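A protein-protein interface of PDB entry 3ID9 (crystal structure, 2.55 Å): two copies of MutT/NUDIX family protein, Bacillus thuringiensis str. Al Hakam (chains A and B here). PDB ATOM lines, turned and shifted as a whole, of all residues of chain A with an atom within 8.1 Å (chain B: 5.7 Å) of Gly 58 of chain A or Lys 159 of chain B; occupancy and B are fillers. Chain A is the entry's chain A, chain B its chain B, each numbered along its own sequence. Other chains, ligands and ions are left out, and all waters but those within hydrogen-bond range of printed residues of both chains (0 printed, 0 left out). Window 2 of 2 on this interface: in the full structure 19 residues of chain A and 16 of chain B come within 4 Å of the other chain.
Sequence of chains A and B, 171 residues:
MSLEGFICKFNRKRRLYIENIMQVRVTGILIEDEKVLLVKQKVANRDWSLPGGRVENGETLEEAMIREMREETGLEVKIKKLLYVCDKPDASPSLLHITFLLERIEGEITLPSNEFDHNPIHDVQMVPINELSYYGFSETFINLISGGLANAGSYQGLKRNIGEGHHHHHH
O of Gly 58 of chain A lies within hydrogen-bond range of NZ of Lys 159 of chain B (2.8 Å). N of Leu 61 of chain A sits at hydrogen-bond distance from OD2 of Asp 87 of chain B (3.0 Å).
NZ of Lys 159 of chain B lies within salt-bridge range of OD1 of Asp 90 of chain B. The backbone carbonyl oxygen (O) of Pro 89 of chain B is in hydrogen-bond range of the side-chain hydroxyl (OG) of Ser 94 of chain B. The backbone NH (N) of Leu 158 of chain B sits at hydrogen-bond distance from the backbone carbonyl oxygen (O) of Asp 87 of chain B, 2.9 Å away. The backbone NH (N) of Glu 56 of chain A lies within hydrogen-bond range of the side-chain carboxylate (OE1) of Glu 59 of chain A (2.7 Å). The side-chain carboxylate (OE1) of Glu 63 of chain A lies within hydrogen-bond range of the backbone NH (N) of Thr 60 of chain A, at 3.0 Å.
C of Gly 58 of chain A touches CB of Pro 89 of chain B, at 3.7 Å. Pro 89 of chain B touches Glu 59 of chain A. OD2 of Asp 87 of chain B touches CA of Thr 60 of chain A, at 3.1 Å. Thr 60 of chain A touches Pro 89 of chain B (CG2 to CG, 3.7 Å). Thr 60 of chain A touches Gly 157 of chain B (CG2 to CA, 3.98 Å). CG2 of Thr 60 of chain A touches CG of Lys 159 of chain B, at 3.5 Å. Lys 159 of chain B touches Glu 63 of chain A.
Of chain B, only Pro 89 and Lys 159 come within 4 Å of Gly 58 of chain A. Printed residues of chain A within 4 Å of Lys 159 of chain B: Gly 58 (2.8 Å), Thr 60 (3.5 Å) and Glu 63 (3.2 Å). Printed residues of chain B within 4 Å of Glu 63 of chain A: Lys 159 (3.2 Å). Of the printed residues of chain A, Gly 157 of chain B touches Thr 60 (3.98 Å). Of the printed residues of chain B, Glu 59 of chain A touches Pro 89 (3.4 Å). Asn 161 of chain B touches none of the printed residues of chain A. Val 55 of chain A touches none of the printed residues of chain B. The nearest residue of chain B that does not touch Gly 58 of chain A is Asp 90 of chain B (4.5 Å).
Of the 9 printed residues of chain A, 5 touch a printed residue of chain B. Printed residues of chain A that touch a printed residue of chain B: Gly 58, Glu 59, Thr 60, Leu 61 and Glu 63. Hydrophobic or aromatic side chains of chain A that line the printed part of chain B: Leu 61. Printed residues of chain B that touch a printed residue of chain A: Asp 87, Pro 89, Gly 157 and Lys 159. Among the printed residues, no Asp or Glu carboxylate lies within 4 Å of a Lys or Arg side-chain nitrogen of the other chain.
No position is printed for both chains.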
ATOM      1  N   VAL A  55      -2.394  33.069 -14.270  1.00  0.00           N
ATOM      2  CA  VAL A  55      -2.989  32.118 -13.350  1.00  0.00           C
ATOM      3  C   VAL A  55      -3.107  32.883 -12.039  1.00  0.00           C
ATOM      4  O   VAL A  55      -2.157  33.533 -11.590  1.00  0.00           O
ATOM      5  CB  VAL A  55      -2.095  30.876 -13.157  1.00  0.00           C
ATOM      6  CG1 VAL A  55      -2.711  29.939 -12.119  1.00  0.00           C
ATOM      7  CG2 VAL A  55      -1.931  30.152 -14.491  1.00  0.00           C
ATOM      8  N   GLU A  56      -4.285  32.833 -11.438  1.00  0.00           N
ATOM      9  CA  GLU A  56      -4.506  33.553 -10.200  1.00  0.00           C
ATOM     10  C   GLU A  56      -4.257  32.731  -8.949  1.00  0.00           C
ATOM     11  O   GLU A  56      -4.371  31.506  -8.961  1.00  0.00           O
ATOM     12  CB  GLU A  56      -5.919  34.139 -10.197  1.00  0.00           C
ATOM     13  CG  GLU A  56      -6.019  35.428 -11.018  1.00  0.00           C
ATOM     14  CD  GLU A  56      -7.452  35.829 -11.335  1.00  0.00           C
ATOM     15  OE1 GLU A  56      -8.340  35.632 -10.472  1.00  0.00           O
ATOM     16  OE2 GLU A  56      -7.689  36.352 -12.450  1.00  0.00           O
ATOM     17  N   ASN A  57      -3.902  33.426  -7.872  1.00  0.00           N
ATOM     18  CA  ASN A  57      -3.619  32.798  -6.588  1.00  0.00           C
ATOM     19  C   ASN A  57      -4.689  31.779  -6.221  1.00  0.00           C
ATOM     20  O   ASN A  57      -5.882  32.084  -6.209  1.00  0.00           O
ATOM     21  CB  ASN A  57      -3.514  33.869  -5.501  1.00  0.00           C
ATOM     22  CG  ASN A  57      -3.017  33.311  -4.178  1.00  0.00           C
ATOM     23  OD1 ASN A  57      -3.774  32.692  -3.423  1.00  0.00           O
ATOM     24  ND2 ASN A  57      -1.730  33.514  -3.896  1.00  0.00           N
ATOM     25  N   GLY A  58      -4.251  30.555  -5.939  1.00  0.00           N
ATOM     26  CA  GLY A  58      -5.175  29.496  -5.583  1.00  0.00           C
ATOM     27  C   GLY A  58      -5.698  28.687  -6.758  1.00  0.00           C
ATOM     28  O   GLY A  58      -6.428  27.714  -6.572  1.00  0.00           O
ATOM     29  N   GLU A  59      -5.330  29.072  -7.972  1.00  0.00           N
ATOM     30  CA  GLU A  59      -5.809  28.358  -9.153  1.00  0.00           C
ATOM     31  C   GLU A  59      -4.847  27.323  -9.706  1.00  0.00           C
ATOM     32  O   GLU A  59      -3.633  27.523  -9.712  1.00  0.00           O
ATOM     33  CB  GLU A  59      -6.099  29.329 -10.298  1.00  0.00           C
ATOM     34  CG  GLU A  59      -7.230  30.298 -10.099  1.00  0.00           C
ATOM     35  CD  GLU A  59      -7.545  31.051 -11.385  1.00  0.00           C
ATOM     36  OE1 GLU A  59      -6.614  31.640 -11.974  1.00  0.00           O
ATOM     37  OE2 GLU A  59      -8.719  31.052 -11.807  1.00  0.00           O
ATOM     38  N   THR A  60      -5.391  26.210 -10.172  1.00  0.00           N
ATOM     39  CA  THR A  60      -4.551  25.218 -10.816  1.00  0.00           C
ATOM     40  C   THR A  60      -4.417  25.807 -12.229  1.00  0.00           C
ATOM     41  O   THR A  60      -5.173  26.716 -12.608  1.00  0.00           O
ATOM     42  CB  THR A  60      -5.240  23.847 -10.915  1.00  0.00           C
ATOM     43  OG1 THR A  60      -6.469  23.977 -11.639  1.00  0.00           O
ATOM     44  CG2 THR A  60      -5.535  23.292  -9.533  1.00  0.00           C
ATOM     45  N   LEU A  61      -3.461  25.327 -13.006  1.00  0.00           N
ATOM     46  CA  LEU A  61      -3.322  25.841 -14.361  1.00  0.00           C
ATOM     47  C   LEU A  61      -4.648  25.640 -15.101  1.00  0.00           C
ATOM     48  O   LEU A  61      -5.091  26.510 -15.844  1.00  0.00           O
ATOM     49  CB  LEU A  61      -2.202  25.106 -15.103  1.00  0.00           C
ATOM     50  CG  LEU A  61      -0.812  25.176 -14.470  1.00  0.00           C
ATOM     51  CD1 LEU A  61       0.192  24.543 -15.426  1.00  0.00           C
ATOM     52  CD2 LEU A  61      -0.439  26.626 -14.178  1.00  0.00           C
ATOM     53  N   GLU A  63      -7.840  25.454 -13.905  1.00  0.00           N
ATOM     54  CA  GLU A  63      -8.912  26.366 -13.526  1.00  0.00           C
ATOM     55  C   GLU A  63      -8.726  27.714 -14.207  1.00  0.00           C
ATOM     56  O   GLU A  63      -9.697  28.327 -14.647  1.00  0.00           O
ATOM     57  CB  GLU A  63      -8.966  26.546 -12.007  1.00  0.00           C
ATOM     58  CG  GLU A  63      -9.349  25.261 -11.282  1.00  0.00           C
ATOM     59  CD  GLU A  63      -9.283  25.391  -9.773  1.00  0.00           C
ATOM     60  OE1 GLU A  63      -8.260  25.894  -9.261  1.00  0.00           O
ATOM     61  OE2 GLU A  63     -10.253  24.979  -9.108  1.00  0.00           O
ATOM     62  N   ALA A  64      -7.479  28.164 -14.302  1.00  0.00           N
ATOM     63  CA  ALA A  64      -7.179  29.433 -14.945  1.00  0.00           C
ATOM     64  C   ALA A  64      -7.533  29.354 -16.428  1.00  0.00           C
ATOM     65  O   ALA A  64      -8.154  30.262 -16.975  1.00  0.00           O
ATOM     66  CB  ALA A  64      -5.705  29.776 -14.777  1.00  0.00           C
ATOM     67  N   ASP B  87       0.419  20.355 -10.521  1.00  0.00           N
ATOM     68  CA  ASP B  87       0.442  21.563  -9.726  1.00  0.00           C
ATOM     69  C   ASP B  87      -0.527  21.521  -8.561  1.00  0.00           C
ATOM     70  O   ASP B  87      -1.638  21.006  -8.670  1.00  0.00           O
ATOM     71  CB  ASP B  87       0.254  22.822 -10.605  1.00  0.00           C
ATOM     72  CG  ASP B  87      -1.178  23.046 -11.056  1.00  0.00           C
ATOM     73  OD1 ASP B  87      -1.801  22.132 -11.637  1.00  0.00           O
ATOM     74  OD2 ASP B  87      -1.671  24.172 -10.840  1.00  0.00           O
ATOM     75  N   PRO B  89      -1.725  24.327  -6.200  1.00  0.00           N
ATOM     76  CA  PRO B  89      -1.758  25.724  -5.765  1.00  0.00           C
ATOM     77  C   PRO B  89      -2.033  25.908  -4.265  1.00  0.00           C
ATOM     78  O   PRO B  89      -1.592  26.899  -3.679  1.00  0.00           O
ATOM     79  CB  PRO B  89      -2.830  26.347  -6.669  1.00  0.00           C
ATOM     80  CG  PRO B  89      -3.733  25.197  -6.977  1.00  0.00           C
ATOM     81  CD  PRO B  89      -2.764  24.057  -7.210  1.00  0.00           C
ATOM     82  N   ASP B  90      -2.732  24.951  -3.644  1.00  0.00           N
ATOM     83  CA  ASP B  90      -3.043  25.048  -2.214  1.00  0.00           C
ATOM     84  C   ASP B  90      -1.861  24.730  -1.293  1.00  0.00           C
ATOM     85  O   ASP B  90      -1.937  24.974  -0.090  1.00  0.00           O
ATOM     86  CB  ASP B  90      -4.211  24.124  -1.820  1.00  0.00           C
ATOM     87  CG  ASP B  90      -5.521  24.485  -2.509  1.00  0.00           C
ATOM     88  OD1 ASP B  90      -5.866  25.688  -2.587  1.00  0.00           O
ATOM     89  OD2 ASP B  90      -6.217  23.549  -2.965  1.00  0.00           O
ATOM     90  N   SER B  94       2.868  27.411  -3.018  1.00  0.00           N
ATOM     91  CA  SER B  94       2.254  26.802  -4.198  1.00  0.00           C
ATOM     92  C   SER B  94       3.297  25.932  -4.873  1.00  0.00           C
ATOM     93  O   SER B  94       4.459  26.320  -4.974  1.00  0.00           O
ATOM     94  CB  SER B  94       1.770  27.874  -5.178  1.00  0.00           C
ATOM     95  OG  SER B  94       0.555  28.447  -4.736  1.00  0.00           O
ATOM     96  N   GLY B 157      -4.160  18.869 -12.177  1.00  0.00           N
ATOM     97  CA  GLY B 157      -4.227  19.898 -11.157  1.00  0.00           C
ATOM     98  C   GLY B 157      -4.784  19.239  -9.907  1.00  0.00           C
ATOM     99  O   GLY B 157      -5.745  18.476  -9.985  1.00  0.00           O
ATOM    100  N   LEU B 158      -4.181  19.517  -8.757  1.00  0.00           N
ATOM    101  CA  LEU B 158      -4.636  18.925  -7.503  1.00  0.00           C
ATOM    102  C   LEU B 158      -4.940  19.966  -6.441  1.00  0.00           C
ATOM    103  O   LEU B 158      -4.089  20.783  -6.088  1.00  0.00           O
ATOM    104  CB  LEU B 158      -3.579  17.966  -6.964  1.00  0.00           C
ATOM    105  CG  LEU B 158      -3.269  16.759  -7.840  1.00  0.00           C
ATOM    106  CD1 LEU B 158      -2.023  16.059  -7.341  1.00  0.00           C
ATOM    107  CD2 LEU B 158      -4.464  15.827  -7.834  1.00  0.00           C
ATOM    108  N   LYS B 159      -6.163  19.922  -5.930  1.00  0.00           N
ATOM    109  CA  LYS B 159      -6.600  20.831  -4.884  1.00  0.00           C
ATOM    110  C   LYS B 159      -7.207  20.000  -3.761  1.00  0.00           C
ATOM    111  O   LYS B 159      -7.745  18.920  -4.008  1.00  0.00           O
ATOM    112  CB  LYS B 159      -7.643  21.810  -5.429  1.00  0.00           C
ATOM    113  CG  LYS B 159      -7.098  22.777  -6.466  1.00  0.00           C
ATOM    114  CD  LYS B 159      -8.144  23.783  -6.925  1.00  0.00           C
ATOM    115  CE  LYS B 159      -8.609  24.687  -5.796  1.00  0.00           C
ATOM    116  NZ  LYS B 159      -7.506  25.513  -5.243  1.00  0.00           N
ATOM    117  N   ARG B 160      -7.103  20.488  -2.530  1.00  0.00           N
ATOM    118  CA  ARG B 160      -7.675  19.772  -1.397  1.00  0.00           C
ATOM    119  C   ARG B 160      -9.196  19.874  -1.419  1.00  0.00           C
ATOM    120  O   ARG B 160      -9.766  20.768  -2.046  1.00  0.00           O
ATOM    121  CB  ARG B 160      -7.143  20.335  -0.076  1.00  0.00           C
ATOM    122  CG  ARG B 160      -5.874  19.670   0.429  1.00  0.00           C
ATOM    123  CD  ARG B 160      -6.127  18.214   0.833  1.00  0.00           C
ATOM    124  NE  ARG B 160      -5.971  18.001   2.275  1.00  0.00           N
ATOM    125  CZ  ARG B 160      -6.974  17.914   3.143  1.00  0.00           C
ATOM    126  NH1 ARG B 160      -8.232  18.016   2.732  1.00  0.00           N
ATOM    127  NH2 ARG B 160      -6.717  17.725   4.432  1.00  0.00           N
ATOM    128  N   ASN B 161      -9.839  18.939  -0.726  1.00  0.00           N
ATOM    129  CA  ASN B 161     -11.298  18.863  -0.621  1.00  0.00           C
ATOM    130  C   ASN B 161     -11.945  18.293  -1.882  1.00  0.00           C
ATOM    131  O   ASN B 161     -11.254  18.183  -2.923  1.00  0.00           O
ATOM    132  CB  ASN B 161     -11.883  20.246  -0.313  1.00  0.00           C
ATOM    133  CG  ASN B 161     -11.116  20.969   0.779  1.00  0.00           C
ATOM    134  OD1 ASN B 161     -10.781  20.386   1.812  1.00  0.00           O
ATOM    135  ND2 ASN B 161     -10.836  22.247   0.557  1.00  0.00           N
